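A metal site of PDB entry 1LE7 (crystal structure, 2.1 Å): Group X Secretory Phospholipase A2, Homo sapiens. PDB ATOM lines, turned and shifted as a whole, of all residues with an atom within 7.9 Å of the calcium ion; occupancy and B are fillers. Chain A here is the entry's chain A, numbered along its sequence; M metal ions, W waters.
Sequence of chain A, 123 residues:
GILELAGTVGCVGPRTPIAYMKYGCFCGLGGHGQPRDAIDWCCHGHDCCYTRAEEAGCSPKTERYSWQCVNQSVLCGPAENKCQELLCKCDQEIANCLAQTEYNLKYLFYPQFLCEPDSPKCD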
ATOM      1  N   TYR A  20     -12.202   7.209  -2.085  1.00  0.00           N
ATOM      2  CA  TYR A  20     -10.777   6.999  -2.344  1.00  0.00           C
ATOM      3  C   TYR A  20     -10.112   8.175  -3.061  1.00  0.00           C
ATOM      4  O   TYR A  20      -8.965   8.085  -3.465  1.00  0.00           O
ATOM      5  CB  TYR A  20     -10.567   5.738  -3.183  1.00  0.00           C
ATOM      6  CG  TYR A  20     -11.407   4.549  -2.753  1.00  0.00           C
ATOM      7  CD1 TYR A  20     -12.562   4.202  -3.446  1.00  0.00           C
ATOM      8  CD2 TYR A  20     -11.025   3.755  -1.670  1.00  0.00           C
ATOM      9  CE1 TYR A  20     -13.317   3.078  -3.091  1.00  0.00           C
ATOM     10  CE2 TYR A  20     -11.775   2.618  -1.306  1.00  0.00           C
ATOM     11  CZ  TYR A  20     -12.919   2.295  -2.023  1.00  0.00           C
ATOM     12  OH  TYR A  20     -13.653   1.178  -1.695  1.00  0.00           O
ATOM     13  N   MET A  21     -10.853   9.271  -3.208  1.00  0.00           N
ATOM     14  CA  MET A  21     -10.337  10.460  -3.879  1.00  0.00           C
ATOM     15  C   MET A  21      -8.997  10.900  -3.308  1.00  0.00           C
ATOM     16  O   MET A  21      -8.072  11.245  -4.053  1.00  0.00           O
ATOM     17  CB  MET A  21     -11.373  11.580  -3.741  1.00  0.00           C
ATOM     18  CG  MET A  21     -11.155  12.768  -4.639  1.00  0.00           C
ATOM     19  SD  MET A  21     -12.615  13.810  -4.590  1.00  0.00           S
ATOM     20  CE  MET A  21     -12.678  14.217  -2.826  1.00  0.00           C
ATOM     21  N   TYR A  23      -6.835   9.352  -0.038  1.00  0.00           N
ATOM     22  CA  TYR A  23      -6.748   8.416   1.072  1.00  0.00           C
ATOM     23  C   TYR A  23      -5.339   7.827   1.166  1.00  0.00           C
ATOM     24  O   TYR A  23      -4.701   7.560   0.151  1.00  0.00           O
ATOM     25  CB  TYR A  23      -7.797   7.325   0.836  1.00  0.00           C
ATOM     26  CG  TYR A  23      -7.924   6.232   1.892  1.00  0.00           C
ATOM     27  CD1 TYR A  23      -6.960   5.237   2.012  1.00  0.00           C
ATOM     28  CD2 TYR A  23      -9.060   6.147   2.695  1.00  0.00           C
ATOM     29  CE1 TYR A  23      -7.116   4.175   2.899  1.00  0.00           C
ATOM     30  CE2 TYR A  23      -9.232   5.095   3.585  1.00  0.00           C
ATOM     31  CZ  TYR A  23      -8.254   4.111   3.680  1.00  0.00           C
ATOM     32  OH  TYR A  23      -8.431   3.058   4.551  1.00  0.00           O
ATOM     33  N   CYS A  25      -1.344   7.100   1.562  1.00  0.00           N
ATOM     34  CA  CYS A  25      -0.215   7.716   0.888  1.00  0.00           C
ATOM     35  C   CYS A  25      -0.266   7.643  -0.631  1.00  0.00           C
ATOM     36  O   CYS A  25       0.497   8.340  -1.304  1.00  0.00           O
ATOM     37  CB  CYS A  25       1.102   7.085   1.346  1.00  0.00           C
ATOM     38  SG  CYS A  25       1.480   7.444   3.080  1.00  0.00           S
ATOM     39  N   PHE A  26      -1.170   6.832  -1.163  1.00  0.00           N
ATOM     40  CA  PHE A  26      -1.241   6.702  -2.612  1.00  0.00           C
ATOM     41  C   PHE A  26      -2.533   6.976  -3.335  1.00  0.00           C
ATOM     42  O   PHE A  26      -2.533   7.096  -4.547  1.00  0.00           O
ATOM     43  CB  PHE A  26      -0.750   5.313  -3.037  1.00  0.00           C
ATOM     44  CG  PHE A  26       0.712   5.123  -2.833  1.00  0.00           C
ATOM     45  CD1 PHE A  26       1.202   4.691  -1.610  1.00  0.00           C
ATOM     46  CD2 PHE A  26       1.593   5.416  -3.863  1.00  0.00           C
ATOM     47  CE1 PHE A  26       2.572   4.565  -1.407  1.00  0.00           C
ATOM     48  CE2 PHE A  26       2.976   5.293  -3.664  1.00  0.00           C
ATOM     49  CZ  PHE A  26       3.460   4.866  -2.429  1.00  0.00           C
ATOM     50  N   CYS A  27      -3.660   7.077  -2.637  1.00  0.00           N
ATOM     51  CA  CYS A  27      -4.885   7.346  -3.367  1.00  0.00           C
ATOM     52  C   CYS A  27      -5.034   8.857  -3.545  1.00  0.00           C
ATOM     53  O   CYS A  27      -5.262   9.601  -2.592  1.00  0.00           O
ATOM     54  CB  CYS A  27      -6.089   6.740  -2.623  1.00  0.00           C
ATOM     55  SG  CYS A  27      -5.953   4.947  -2.252  1.00  0.00           S
ATOM     56  N   GLY A  28      -4.900   9.303  -4.785  1.00  0.00           N
ATOM     57  CA  GLY A  28      -4.977  10.724  -5.099  1.00  0.00           C
ATOM     58  C   GLY A  28      -3.788  11.057  -5.969  1.00  0.00           C
ATOM     59  O   GLY A  28      -2.856  10.282  -6.018  1.00  0.00           O
ATOM     60  N   LEU A  29      -3.798  12.221  -6.635  1.00  0.00           N
ATOM     61  CA  LEU A  29      -2.693  12.613  -7.509  1.00  0.00           C
ATOM     62  C   LEU A  29      -1.327  12.308  -6.915  1.00  0.00           C
ATOM     63  O   LEU A  29      -1.029  12.710  -5.803  1.00  0.00           O
ATOM     64  CB  LEU A  29      -2.799  14.107  -7.830  1.00  0.00           C
ATOM     65  CG  LEU A  29      -1.903  14.645  -8.939  1.00  0.00           C
ATOM     66  CD1 LEU A  29      -2.265  13.980 -10.269  1.00  0.00           C
ATOM     67  CD2 LEU A  29      -2.075  16.156  -9.060  1.00  0.00           C
ATOM     68  N   GLY A  30      -0.494  11.593  -7.674  1.00  0.00           N
ATOM     69  CA  GLY A  30       0.843  11.245  -7.205  1.00  0.00           C
ATOM     70  C   GLY A  30       0.835  10.334  -6.001  1.00  0.00           C
ATOM     71  O   GLY A  30      -0.140   9.616  -5.770  1.00  0.00           O
ATOM     72  N   GLY A  31       1.898  10.344  -5.207  1.00  0.00           N
ATOM     73  CA  GLY A  31       1.947   9.515  -4.021  1.00  0.00           C
ATOM     74  C   GLY A  31       3.314   8.949  -3.743  1.00  0.00           C
ATOM     75  O   GLY A  31       4.079   8.664  -4.664  1.00  0.00           O
ATOM     76  N   HIS A  32       3.640   8.774  -2.463  1.00  0.00           N
ATOM     77  CA  HIS A  32       4.935   8.226  -2.066  1.00  0.00           C
ATOM     78  C   HIS A  32       4.877   7.702  -0.634  1.00  0.00           C
ATOM     79  O   HIS A  32       3.958   8.045   0.125  1.00  0.00           O
ATOM     80  CB  HIS A  32       6.029   9.295  -2.179  1.00  0.00           C
ATOM     81  CG  HIS A  32       5.766  10.512  -1.357  1.00  0.00           C
ATOM     82  ND1 HIS A  32       5.010  11.571  -1.808  1.00  0.00           N
ATOM     83  CD2 HIS A  32       6.127  10.827  -0.090  1.00  0.00           C
ATOM     84  CE1 HIS A  32       4.917  12.481  -0.865  1.00  0.00           C
ATOM     85  NE2 HIS A  32       5.580  12.057   0.192  1.00  0.00           N
ATOM     86  N   ASP A  40      -4.681   1.426   0.307  1.00  0.00           N
ATOM     87  CA  ASP A  40      -3.527   2.199  -0.135  1.00  0.00           C
ATOM     88  C   ASP A  40      -2.658   1.349  -1.071  1.00  0.00           C
ATOM     89  O   ASP A  40      -1.999   1.876  -1.968  1.00  0.00           O
ATOM     90  CB  ASP A  40      -2.728   2.663   1.080  1.00  0.00           C
ATOM     91  CG  ASP A  40      -2.019   4.000   0.849  1.00  0.00           C
ATOM     92  OD1 ASP A  40      -2.324   4.674  -0.143  1.00  0.00           O
ATOM     93  OD2 ASP A  40      -1.153   4.360   1.662  1.00  0.00           O
ATOM     94  N   CYS A  43      -4.118   1.414  -4.565  1.00  0.00           N
ATOM     95  CA  CYS A  43      -3.773   2.647  -5.270  1.00  0.00           C
ATOM     96  C   CYS A  43      -2.318   2.643  -5.702  1.00  0.00           C
ATOM     97  O   CYS A  43      -1.955   3.234  -6.726  1.00  0.00           O
ATOM     98  CB  CYS A  43      -4.088   3.858  -4.393  1.00  0.00           C
ATOM     99  SG  CYS A  43      -5.862   4.037  -4.059  1.00  0.00           S
ATOM    100  N   HIS A  44      -1.468   1.963  -4.943  1.00  0.00           N
ATOM    101  CA  HIS A  44      -0.052   1.883  -5.279  1.00  0.00           C
ATOM    102  C   HIS A  44       0.079   1.118  -6.578  1.00  0.00           C
ATOM    103  O   HIS A  44       0.748   1.552  -7.503  1.00  0.00           O
ATOM    104  CB  HIS A  44       0.743   1.172  -4.176  1.00  0.00           C
ATOM    105  CG  HIS A  44       2.183   0.974  -4.511  1.00  0.00           C
ATOM    106  ND1 HIS A  44       2.644  -0.151  -5.170  1.00  0.00           N
ATOM    107  CD2 HIS A  44       3.259   1.780  -4.339  1.00  0.00           C
ATOM    108  CE1 HIS A  44       3.948  -0.027  -5.387  1.00  0.00           C
ATOM    109  NE2 HIS A  44       4.345   1.136  -4.895  1.00  0.00           N
ATOM    110  N   HIS A  46      -2.161   0.651  -8.764  1.00  0.00           N
ATOM    111  CA  HIS A  46      -2.823   1.374  -9.838  1.00  0.00           C
ATOM    112  C   HIS A  46      -1.860   2.421 -10.403  1.00  0.00           C
ATOM    113  O   HIS A  46      -1.719   2.555 -11.608  1.00  0.00           O
ATOM    114  CB  HIS A  46      -4.117   2.002  -9.324  1.00  0.00           C
ATOM    115  CG  HIS A  46      -4.952   2.652 -10.383  1.00  0.00           C
ATOM    116  ND1 HIS A  46      -5.079   4.022 -10.497  1.00  0.00           N
ATOM    117  CD2 HIS A  46      -5.730   2.118 -11.352  1.00  0.00           C
ATOM    118  CE1 HIS A  46      -5.899   4.302 -11.489  1.00  0.00           C
ATOM    119  NE2 HIS A  46      -6.310   3.173 -12.030  1.00  0.00           N
ATOM    120  N   ASP A  47      -1.188   3.162  -9.522  1.00  0.00           N
ATOM    121  CA  ASP A  47      -0.231   4.162  -9.980  1.00  0.00           C
ATOM    122  C   ASP A  47       0.791   3.489 -10.870  1.00  0.00           C
ATOM    123  O   ASP A  47       1.106   3.966 -11.960  1.00  0.00           O
ATOM    124  CB  ASP A  47       0.501   4.799  -8.790  1.00  0.00           C
ATOM    125  CG  ASP A  47      -0.397   5.701  -7.973  1.00  0.00           C
ATOM    126  OD1 ASP A  47       0.104   6.302  -6.992  1.00  0.00           O
ATOM    127  OD2 ASP A  47      -1.601   5.804  -8.286  1.00  0.00           O
ATOM    128  N   CYS A  48       1.323   2.366 -10.393  1.00  0.00           N
ATOM    129  CA  CYS A  48       2.303   1.623 -11.166  1.00  0.00           C
ATOM    130  C   CYS A  48       1.748   1.303 -12.550  1.00  0.00           C
ATOM    131  O   CYS A  48       2.402   1.530 -13.564  1.00  0.00           O
ATOM    132  CB  CYS A  48       2.670   0.338 -10.434  1.00  0.00           C
ATOM    133  SG  CYS A  48       3.653   0.533  -8.909  1.00  0.00           S
ATOM    134  N   TYR A  50      -0.637   2.759 -14.216  1.00  0.00           N
ATOM    135  CA  TYR A  50      -0.742   3.972 -15.028  1.00  0.00           C
ATOM    136  C   TYR A  50       0.620   4.412 -15.553  1.00  0.00           C
ATOM    137  O   TYR A  50       0.718   4.900 -16.684  1.00  0.00           O
ATOM    138  CB  TYR A  50      -1.402   5.110 -14.219  1.00  0.00           C
ATOM    139  CG  TYR A  50      -2.917   5.177 -14.373  1.00  0.00           C
ATOM    140  CD1 TYR A  50      -3.649   4.066 -14.798  1.00  0.00           C
ATOM    141  CD2 TYR A  50      -3.618   6.338 -14.060  1.00  0.00           C
ATOM    142  CE1 TYR A  50      -5.049   4.111 -14.906  1.00  0.00           C
ATOM    143  CE2 TYR A  50      -5.011   6.399 -14.182  1.00  0.00           C
ATOM    144  CZ  TYR A  50      -5.718   5.287 -14.602  1.00  0.00           C
ATOM    145  OH  TYR A  50      -7.102   5.350 -14.685  1.00  0.00           O
ATOM    146  N   ILE A  94      -7.835  -2.116 -10.169  1.00  0.00           N
ATOM    147  CA  ILE A  94      -7.952  -1.442  -8.879  1.00  0.00           C
ATOM    148  C   ILE A  94      -9.388  -1.594  -8.351  1.00  0.00           C
ATOM    149  O   ILE A  94      -9.605  -1.660  -7.141  1.00  0.00           O
ATOM    150  CB  ILE A  94      -7.567   0.088  -8.949  1.00  0.00           C
ATOM    151  CG1 ILE A  94      -7.454   0.645  -7.523  1.00  0.00           C
ATOM    152  CG2 ILE A  94      -8.611   0.871  -9.749  1.00  0.00           C
ATOM    153  CD1 ILE A  94      -7.082   2.140  -7.444  1.00  0.00           C
HETATM  154 CA    CA M   1      -1.913   7.982  -6.802  1.00  0.00          CA
HETATM  155  O   HOH W   1      -4.447   7.462  -7.268  1.00  0.00           O
HETATM  156  O   HOH W   2      -1.058   9.009  -9.142  1.00  0.00           O
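The backbone carbonyl oxygen (O) of Phe 26 is bound to the calcium ion. O of Gly 28 binds the calcium ion (2.6 Å). The calcium ion is bound by O of Gly 30 (2.6 Å). Water W1 binds the calcium ion. The side-chain carboxylate (OD1) of Asp 47 binds the calcium ion (2.6 Å). The calcium ion is bound by the side-chain carboxylate (OD2) of Asp 47 (2.7 Å). The calcium ion is bound by water W2, at 2.7 Å. The calcium ion has seven donor atoms within binding distance.
The backbone NH (N) of Phe 26 sits at hydrogen-bond distance from the side-chain carboxylate (OD1) of Asp 40, 2.7 Å away. The side-chain sulfur of Cys 43 is disulfide-bonded to the side-chain sulfur of Cys 27 (2.0 Å).
The nearest printed residue that does not touch the calcium ion is Leu 29 (4.4 Å).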
